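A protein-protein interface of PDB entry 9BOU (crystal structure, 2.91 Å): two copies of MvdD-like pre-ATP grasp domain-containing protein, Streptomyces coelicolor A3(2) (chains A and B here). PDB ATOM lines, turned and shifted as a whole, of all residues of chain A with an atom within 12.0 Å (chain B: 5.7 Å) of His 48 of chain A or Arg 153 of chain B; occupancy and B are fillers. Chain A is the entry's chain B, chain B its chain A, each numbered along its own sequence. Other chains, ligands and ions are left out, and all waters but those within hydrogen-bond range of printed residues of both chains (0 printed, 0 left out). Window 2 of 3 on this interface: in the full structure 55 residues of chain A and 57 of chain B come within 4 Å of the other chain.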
ATOM      1  N   GLY A  44      -3.261   2.199  23.610  1.00  0.00           N
ATOM      2  CA  GLY A  44      -2.627   2.427  22.332  1.00  0.00           C
ATOM      3  C   GLY A  44      -3.452   3.382  21.517  1.00  0.00           C
ATOM      4  O   GLY A  44      -4.630   3.126  21.271  1.00  0.00           O
ATOM      5  N   GLU A  45      -2.852   4.495  21.121  1.00  0.00           N
ATOM      6  CA  GLU A  45      -3.494   5.500  20.288  1.00  0.00           C
ATOM      7  C   GLU A  45      -2.768   5.533  18.951  1.00  0.00           C
ATOM      8  O   GLU A  45      -1.548   5.737  18.920  1.00  0.00           O
ATOM      9  CB  GLU A  45      -3.446   6.866  20.973  1.00  0.00           C
ATOM     10  CG  GLU A  45      -3.887   8.044  20.093  1.00  0.00           C
ATOM     11  CD  GLU A  45      -4.325   9.242  20.917  1.00  0.00           C
ATOM     12  OE1 GLU A  45      -4.244   9.113  22.154  1.00  0.00           O
ATOM     13  OE2 GLU A  45      -4.747  10.287  20.343  1.00  0.00           O
ATOM     14  N   PHE A  46      -3.511   5.306  17.860  1.00  0.00           N
ATOM     15  CA  PHE A  46      -3.031   5.569  16.508  1.00  0.00           C
ATOM     16  C   PHE A  46      -3.657   6.866  16.020  1.00  0.00           C
ATOM     17  O   PHE A  46      -4.857   6.891  15.706  1.00  0.00           O
ATOM     18  CB  PHE A  46      -3.430   4.495  15.503  1.00  0.00           C
ATOM     19  CG  PHE A  46      -3.210   3.110  15.952  1.00  0.00           C
ATOM     20  CD1 PHE A  46      -4.032   2.522  16.901  1.00  0.00           C
ATOM     21  CD2 PHE A  46      -2.206   2.364  15.384  1.00  0.00           C
ATOM     22  CE1 PHE A  46      -3.826   1.219  17.295  1.00  0.00           C
ATOM     23  CE2 PHE A  46      -2.013   1.074  15.759  1.00  0.00           C
ATOM     24  CZ  PHE A  46      -2.828   0.499  16.726  1.00  0.00           C
ATOM     25  N   ALA A  47      -2.857   7.923  15.893  1.00  0.00           N
ATOM     26  CA  ALA A  47      -3.428   9.166  15.390  1.00  0.00           C
ATOM     27  C   ALA A  47      -2.355   9.980  14.688  1.00  0.00           C
ATOM     28  O   ALA A  47      -1.181   9.973  15.076  1.00  0.00           O
ATOM     29  CB  ALA A  47      -4.090   9.982  16.511  1.00  0.00           C
ATOM     30  N   HIS A  48      -2.782  10.681  13.640  1.00  0.00           N
ATOM     31  CA  HIS A  48      -1.895  11.556  12.880  1.00  0.00           C
ATOM     32  C   HIS A  48      -0.713  10.758  12.332  1.00  0.00           C
ATOM     33  O   HIS A  48       0.429  11.242  12.314  1.00  0.00           O
ATOM     34  CB  HIS A  48      -1.414  12.753  13.718  1.00  0.00           C
ATOM     35  CG  HIS A  48      -2.505  13.475  14.454  1.00  0.00           C
ATOM     36  ND1 HIS A  48      -3.804  13.544  13.992  1.00  0.00           N
ATOM     37  CD2 HIS A  48      -2.486  14.152  15.628  1.00  0.00           C
ATOM     38  CE1 HIS A  48      -4.538  14.223  14.856  1.00  0.00           C
ATOM     39  NE2 HIS A  48      -3.761  14.605  15.858  1.00  0.00           N
ATOM     40  N   GLY A  49      -1.001   9.520  11.880  1.00  0.00           N
ATOM     41  CA  GLY A  49      -0.017   8.625  11.297  1.00  0.00           C
ATOM     42  C   GLY A  49       0.917   7.946  12.278  1.00  0.00           C
ATOM     43  O   GLY A  49       1.626   7.018  11.888  1.00  0.00           O
ATOM     44  N   SER A  50       0.944   8.372  13.531  1.00  0.00           N
ATOM     45  CA  SER A  50       1.852   7.853  14.531  1.00  0.00           C
ATOM     46  C   SER A  50       1.141   6.799  15.372  1.00  0.00           C
ATOM     47  O   SER A  50      -0.057   6.539  15.231  1.00  0.00           O
ATOM     48  CB  SER A  50       2.363   9.005  15.393  1.00  0.00           C
ATOM     49  OG  SER A  50       2.808  10.091  14.593  1.00  0.00           O
ATOM     50  N   PHE A  51       1.887   6.197  16.289  1.00  0.00           N
ATOM     51  CA  PHE A  51       1.284   5.339  17.302  1.00  0.00           C
ATOM     52  C   PHE A  51       2.001   5.537  18.617  1.00  0.00           C
ATOM     53  O   PHE A  51       3.225   5.532  18.654  1.00  0.00           O
ATOM     54  CB  PHE A  51       1.361   3.867  16.921  1.00  0.00           C
ATOM     55  CG  PHE A  51       0.983   2.916  18.043  1.00  0.00           C
ATOM     56  CD1 PHE A  51      -0.342   2.533  18.241  1.00  0.00           C
ATOM     57  CD2 PHE A  51       1.947   2.354  18.852  1.00  0.00           C
ATOM     58  CE1 PHE A  51      -0.683   1.630  19.230  1.00  0.00           C
ATOM     59  CE2 PHE A  51       1.604   1.453  19.845  1.00  0.00           C
ATOM     60  CZ  PHE A  51       0.291   1.102  20.030  1.00  0.00           C
ATOM     61  N   ARG A  52       1.262   5.688  19.685  1.00  0.00           N
ATOM     62  CA  ARG A  52       1.818   5.827  21.019  1.00  0.00           C
ATOM     63  C   ARG A  52       1.106   4.781  21.859  1.00  0.00           C
ATOM     64  O   ARG A  52      -0.048   4.447  21.589  1.00  0.00           O
ATOM     65  CB  ARG A  52       1.620   7.243  21.539  1.00  0.00           C
ATOM     66  CG  ARG A  52       2.517   7.625  22.711  1.00  0.00           C
ATOM     67  CD  ARG A  52       2.861   9.129  22.719  1.00  0.00           C
ATOM     68  NE  ARG A  52       2.565   9.766  24.003  1.00  0.00           N
ATOM     69  CZ  ARG A  52       3.303   9.639  25.102  1.00  0.00           C
ATOM     70  NH1 ARG A  52       4.401   8.888  25.120  1.00  0.00           N
ATOM     71  NH2 ARG A  52       2.931  10.280  26.209  1.00  0.00           N
ATOM     72  N   GLN B 129      -1.427   2.718   8.257  1.00  0.00           N
ATOM     73  CA  GLN B 129      -0.691   3.925   8.587  1.00  0.00           C
ATOM     74  C   GLN B 129       0.639   3.978   7.842  1.00  0.00           C
ATOM     75  O   GLN B 129       0.960   4.971   7.181  1.00  0.00           O
ATOM     76  CB  GLN B 129      -0.450   3.954  10.083  1.00  0.00           C
ATOM     77  CG  GLN B 129      -1.257   4.921  10.843  1.00  0.00           C
ATOM     78  CD  GLN B 129      -0.885   4.898  12.312  1.00  0.00           C
ATOM     79  OE1 GLN B 129       0.033   4.170  12.757  1.00  0.00           O
ATOM     80  NE2 GLN B 129      -1.593   5.699  13.082  1.00  0.00           N
ATOM     81  N   VAL B 135      -6.028   6.960   8.517  1.00  0.00           N
ATOM     82  CA  VAL B 135      -6.649   6.177   9.579  1.00  0.00           C
ATOM     83  C   VAL B 135      -7.239   7.081  10.649  1.00  0.00           C
ATOM     84  O   VAL B 135      -6.549   7.967  11.182  1.00  0.00           O
ATOM     85  CB  VAL B 135      -5.625   5.199  10.176  1.00  0.00           C
ATOM     86  CG1 VAL B 135      -6.238   4.375  11.281  1.00  0.00           C
ATOM     87  CG2 VAL B 135      -5.080   4.257   9.130  1.00  0.00           C
ATOM     88  N   ARG B 148     -11.461   8.551  28.734  1.00  0.00           N
ATOM     89  CA  ARG B 148     -12.151   9.812  28.992  1.00  0.00           C
ATOM     90  C   ARG B 148     -11.377  10.992  28.409  1.00  0.00           C
ATOM     91  O   ARG B 148     -11.990  11.932  27.893  1.00  0.00           O
ATOM     92  CB  ARG B 148     -12.453   9.960  30.491  1.00  0.00           C
ATOM     93  CG  ARG B 148     -13.831   9.301  30.835  1.00  0.00           C
ATOM     94  CD  ARG B 148     -14.029   8.873  32.297  1.00  0.00           C
ATOM     95  NE  ARG B 148     -12.983   9.437  33.143  1.00  0.00           N
ATOM     96  CZ  ARG B 148     -12.375   8.788  34.127  1.00  0.00           C
ATOM     97  NH1 ARG B 148     -12.744   7.563  34.482  1.00  0.00           N
ATOM     98  NH2 ARG B 148     -11.368   9.381  34.763  1.00  0.00           N
ATOM     99  N   GLU B 149     -10.041  10.962  28.424  1.00  0.00           N
ATOM    100  CA  GLU B 149      -9.312  12.023  27.736  1.00  0.00           C
ATOM    101  C   GLU B 149      -9.521  11.925  26.235  1.00  0.00           C
ATOM    102  O   GLU B 149      -9.573  12.947  25.553  1.00  0.00           O
ATOM    103  CB  GLU B 149      -7.816  11.963  28.026  1.00  0.00           C
ATOM    104  CG  GLU B 149      -6.942  13.031  27.281  1.00  0.00           C
ATOM    105  CD  GLU B 149      -6.667  12.775  25.760  1.00  0.00           C
ATOM    106  OE1 GLU B 149      -5.987  13.622  25.127  1.00  0.00           O
ATOM    107  OE2 GLU B 149      -7.122  11.771  25.175  1.00  0.00           O
ATOM    108  N   PHE B 150      -9.562  10.699  25.692  1.00  0.00           N
ATOM    109  CA  PHE B 150      -9.722  10.522  24.248  1.00  0.00           C
ATOM    110  C   PHE B 150     -11.043  11.121  23.771  1.00  0.00           C
ATOM    111  O   PHE B 150     -11.081  11.830  22.756  1.00  0.00           O
ATOM    112  CB  PHE B 150      -9.649   9.034  23.865  1.00  0.00           C
ATOM    113  CG  PHE B 150      -9.612   8.797  22.384  1.00  0.00           C
ATOM    114  CD1 PHE B 150      -8.434   8.918  21.677  1.00  0.00           C
ATOM    115  CD2 PHE B 150     -10.758   8.484  21.704  1.00  0.00           C
ATOM    116  CE1 PHE B 150      -8.402   8.728  20.327  1.00  0.00           C
ATOM    117  CE2 PHE B 150     -10.730   8.287  20.350  1.00  0.00           C
ATOM    118  CZ  PHE B 150      -9.554   8.413  19.663  1.00  0.00           C
ATOM    119  N   ALA B 151     -12.138  10.845  24.496  1.00  0.00           N
ATOM    120  CA  ALA B 151     -13.444  11.426  24.161  1.00  0.00           C
ATOM    121  C   ALA B 151     -13.412  12.957  24.214  1.00  0.00           C
ATOM    122  O   ALA B 151     -13.905  13.632  23.302  1.00  0.00           O
ATOM    123  CB  ALA B 151     -14.525  10.877  25.102  1.00  0.00           C
ATOM    124  N   GLU B 152     -12.876  13.521  25.299  1.00  0.00           N
ATOM    125  CA  GLU B 152     -12.531  14.934  25.347  1.00  0.00           C
ATOM    126  C   GLU B 152     -11.953  15.427  24.016  1.00  0.00           C
ATOM    127  O   GLU B 152     -12.525  16.321  23.393  1.00  0.00           O
ATOM    128  CB  GLU B 152     -11.550  15.137  26.508  1.00  0.00           C
ATOM    129  CG  GLU B 152     -11.652  16.464  27.246  1.00  0.00           C
ATOM    130  CD  GLU B 152     -10.306  16.888  27.873  1.00  0.00           C
ATOM    131  OE1 GLU B 152      -9.728  17.891  27.398  1.00  0.00           O
ATOM    132  OE2 GLU B 152      -9.840  16.225  28.834  1.00  0.00           O
ATOM    133  N   ARG B 153     -10.819  14.861  23.561  1.00  0.00           N
ATOM    134  CA  ARG B 153     -10.179  15.334  22.327  1.00  0.00           C
ATOM    135  C   ARG B 153     -11.128  15.172  21.136  1.00  0.00           C
ATOM    136  O   ARG B 153     -11.241  16.076  20.298  1.00  0.00           O
ATOM    137  CB  ARG B 153      -8.860  14.563  22.067  1.00  0.00           C
ATOM    138  CG  ARG B 153      -7.453  15.216  22.399  1.00  0.00           C
ATOM    139  CD  ARG B 153      -6.282  14.682  21.458  1.00  0.00           C
ATOM    140  NE  ARG B 153      -6.293  15.324  20.132  1.00  0.00           N
ATOM    141  CZ  ARG B 153      -5.295  15.341  19.249  1.00  0.00           C
ATOM    142  NH1 ARG B 153      -4.164  14.691  19.462  1.00  0.00           N
ATOM    143  NH2 ARG B 153      -5.437  16.034  18.124  1.00  0.00           N
ATOM    144  N   TYR B 154     -11.818  14.015  21.053  1.00  0.00           N
ATOM    145  CA  TYR B 154     -12.665  13.603  19.921  1.00  0.00           C
ATOM    146  C   TYR B 154     -14.018  13.165  20.488  1.00  0.00           C
ATOM    147  O   TYR B 154     -14.221  11.979  20.776  1.00  0.00           O
ATOM    148  CB  TYR B 154     -12.044  12.429  19.110  1.00  0.00           C
ATOM    149  CG  TYR B 154     -10.644  12.623  18.513  1.00  0.00           C
ATOM    150  CD1 TYR B 154      -9.514  12.583  19.319  1.00  0.00           C
ATOM    151  CD2 TYR B 154     -10.467  12.823  17.148  1.00  0.00           C
ATOM    152  CE1 TYR B 154      -8.252  12.783  18.801  1.00  0.00           C
ATOM    153  CE2 TYR B 154      -9.217  13.024  16.615  1.00  0.00           C
ATOM    154  CZ  TYR B 154      -8.103  13.002  17.445  1.00  0.00           C
ATOM    155  OH  TYR B 154      -6.827  13.194  16.929  1.00  0.00           O
ATOM    156  N   PRO B 155     -14.975  14.078  20.664  1.00  0.00           N
ATOM    157  CA  PRO B 155     -16.274  13.688  21.265  1.00  0.00           C
ATOM    158  C   PRO B 155     -17.264  12.932  20.365  1.00  0.00           C
ATOM    159  O   PRO B 155     -18.270  12.403  20.876  1.00  0.00           O
ATOM    160  CB  PRO B 155     -16.892  15.031  21.690  1.00  0.00           C
ATOM    161  CG  PRO B 155     -15.979  16.102  21.211  1.00  0.00           C
ATOM    162  CD  PRO B 155     -14.800  15.530  20.500  1.00  0.00           C
ATOM    163  N   ARG B 197     -12.646   7.956  16.292  1.00  0.00           N
ATOM    164  CA  ARG B 197     -13.327   9.157  15.815  1.00  0.00           C
ATOM    165  C   ARG B 197     -14.159   8.798  14.585  1.00  0.00           C
ATOM    166  O   ARG B 197     -13.688   8.107  13.674  1.00  0.00           O
ATOM    167  CB  ARG B 197     -12.310  10.279  15.513  1.00  0.00           C
ATOM    168  CG  ARG B 197     -11.719  10.323  14.096  1.00  0.00           C
ATOM    169  CD  ARG B 197     -10.874  11.629  13.772  1.00  0.00           C
ATOM    170  NE  ARG B 197      -9.744  11.349  12.876  1.00  0.00           N
ATOM    171  CZ  ARG B 197      -8.656  12.093  12.742  1.00  0.00           C
ATOM    172  NH1 ARG B 197      -8.514  13.246  13.377  1.00  0.00           N
ATOM    173  NH2 ARG B 197      -7.684  11.663  11.950  1.00  0.00           N
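The side-chain amide oxygen of Gln 129 of chain B lies close to the backbone carbonyl oxygen of Gly 49 of chain A. O of Ser 50 of chain A lies within hydrogen-bond range of NE2 of Gln 129 of chain B, 2.8 Å away. The guanidinium group (NH2) of Arg 153 of chain B is in hydrogen-bond range of a ring nitrogen (NE2) of His 48 of chain A, at 3.2 Å.
Of the 11 printed residues of chain B, 4 touch a printed residue of chain A. Hydrophobic or aromatic side chains of chain A within 4 Å of the printed part of chain B: Phe 46 and His 48. Among the printed residues, 7 pairs touch across the chains. Among the printed residues, no Asp or Glu carboxylate lies within 4 Å of a Lys or Arg side-chain nitrogen of the other chain.
CE1 of Phe 150 of chain B touches OE2 of Glu 45 of chain A (3.97 Å). Gln 129 of chain B touches Phe 46 of chain A. Ala 47 of chain A touches Gln 129 of chain B (N to NE2, 3.8 Å). CE1 of His 48 of chain A touches OH of Tyr 154 of chain B (3.3 Å).
NH2 of Arg 153 of chain B sits at hydrogen-bond distance from OH of Tyr 154 of chain B, at 3.4 Å. The backbone NH (N) of Glu 45 of chain A sits at hydrogen-bond distance from the backbone carbonyl oxygen (O) of Arg 52 of chain A (2.8 Å). The side-chain hydroxyl (OG) of Ser 50 of chain A sits at hydrogen-bond distance from the backbone carbonyl oxygen (O) of His 48 of chain A (3.5 Å).
Printed residues of chain B within 4 Å of Glu 45 of chain A: Phe 150. Printed residues of chain B within 4 Å of Phe 46 of chain A: Gln 129 (3.3 Å). Of the printed residues of chain B, His 48 of chain A touches Arg 153 (3.2 Å) and Tyr 154 (3.3 Å). Printed residues of chain B within 4 Å of Gly 49 of chain A: Gln 129. No residue of chain A comes within 4 Å of Glu 152 of chain B. Of the printed residues of chain A, Arg 153 of chain B touches His 48 (3.2 Å). Tyr 154 of chain B touches just one residue of chain A: His 48. No residue of chain A comes within 4 Å of Pro 155 of chain B. The nearest printed residue of chain A that does not touch Gln 129 of chain B is Phe 51 of chain A (4.4 Å).
No position is printed for both chains. Of the 7 pairs that touch across the chains among the printed residues, none has its exchanged pair printed and touching as well.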
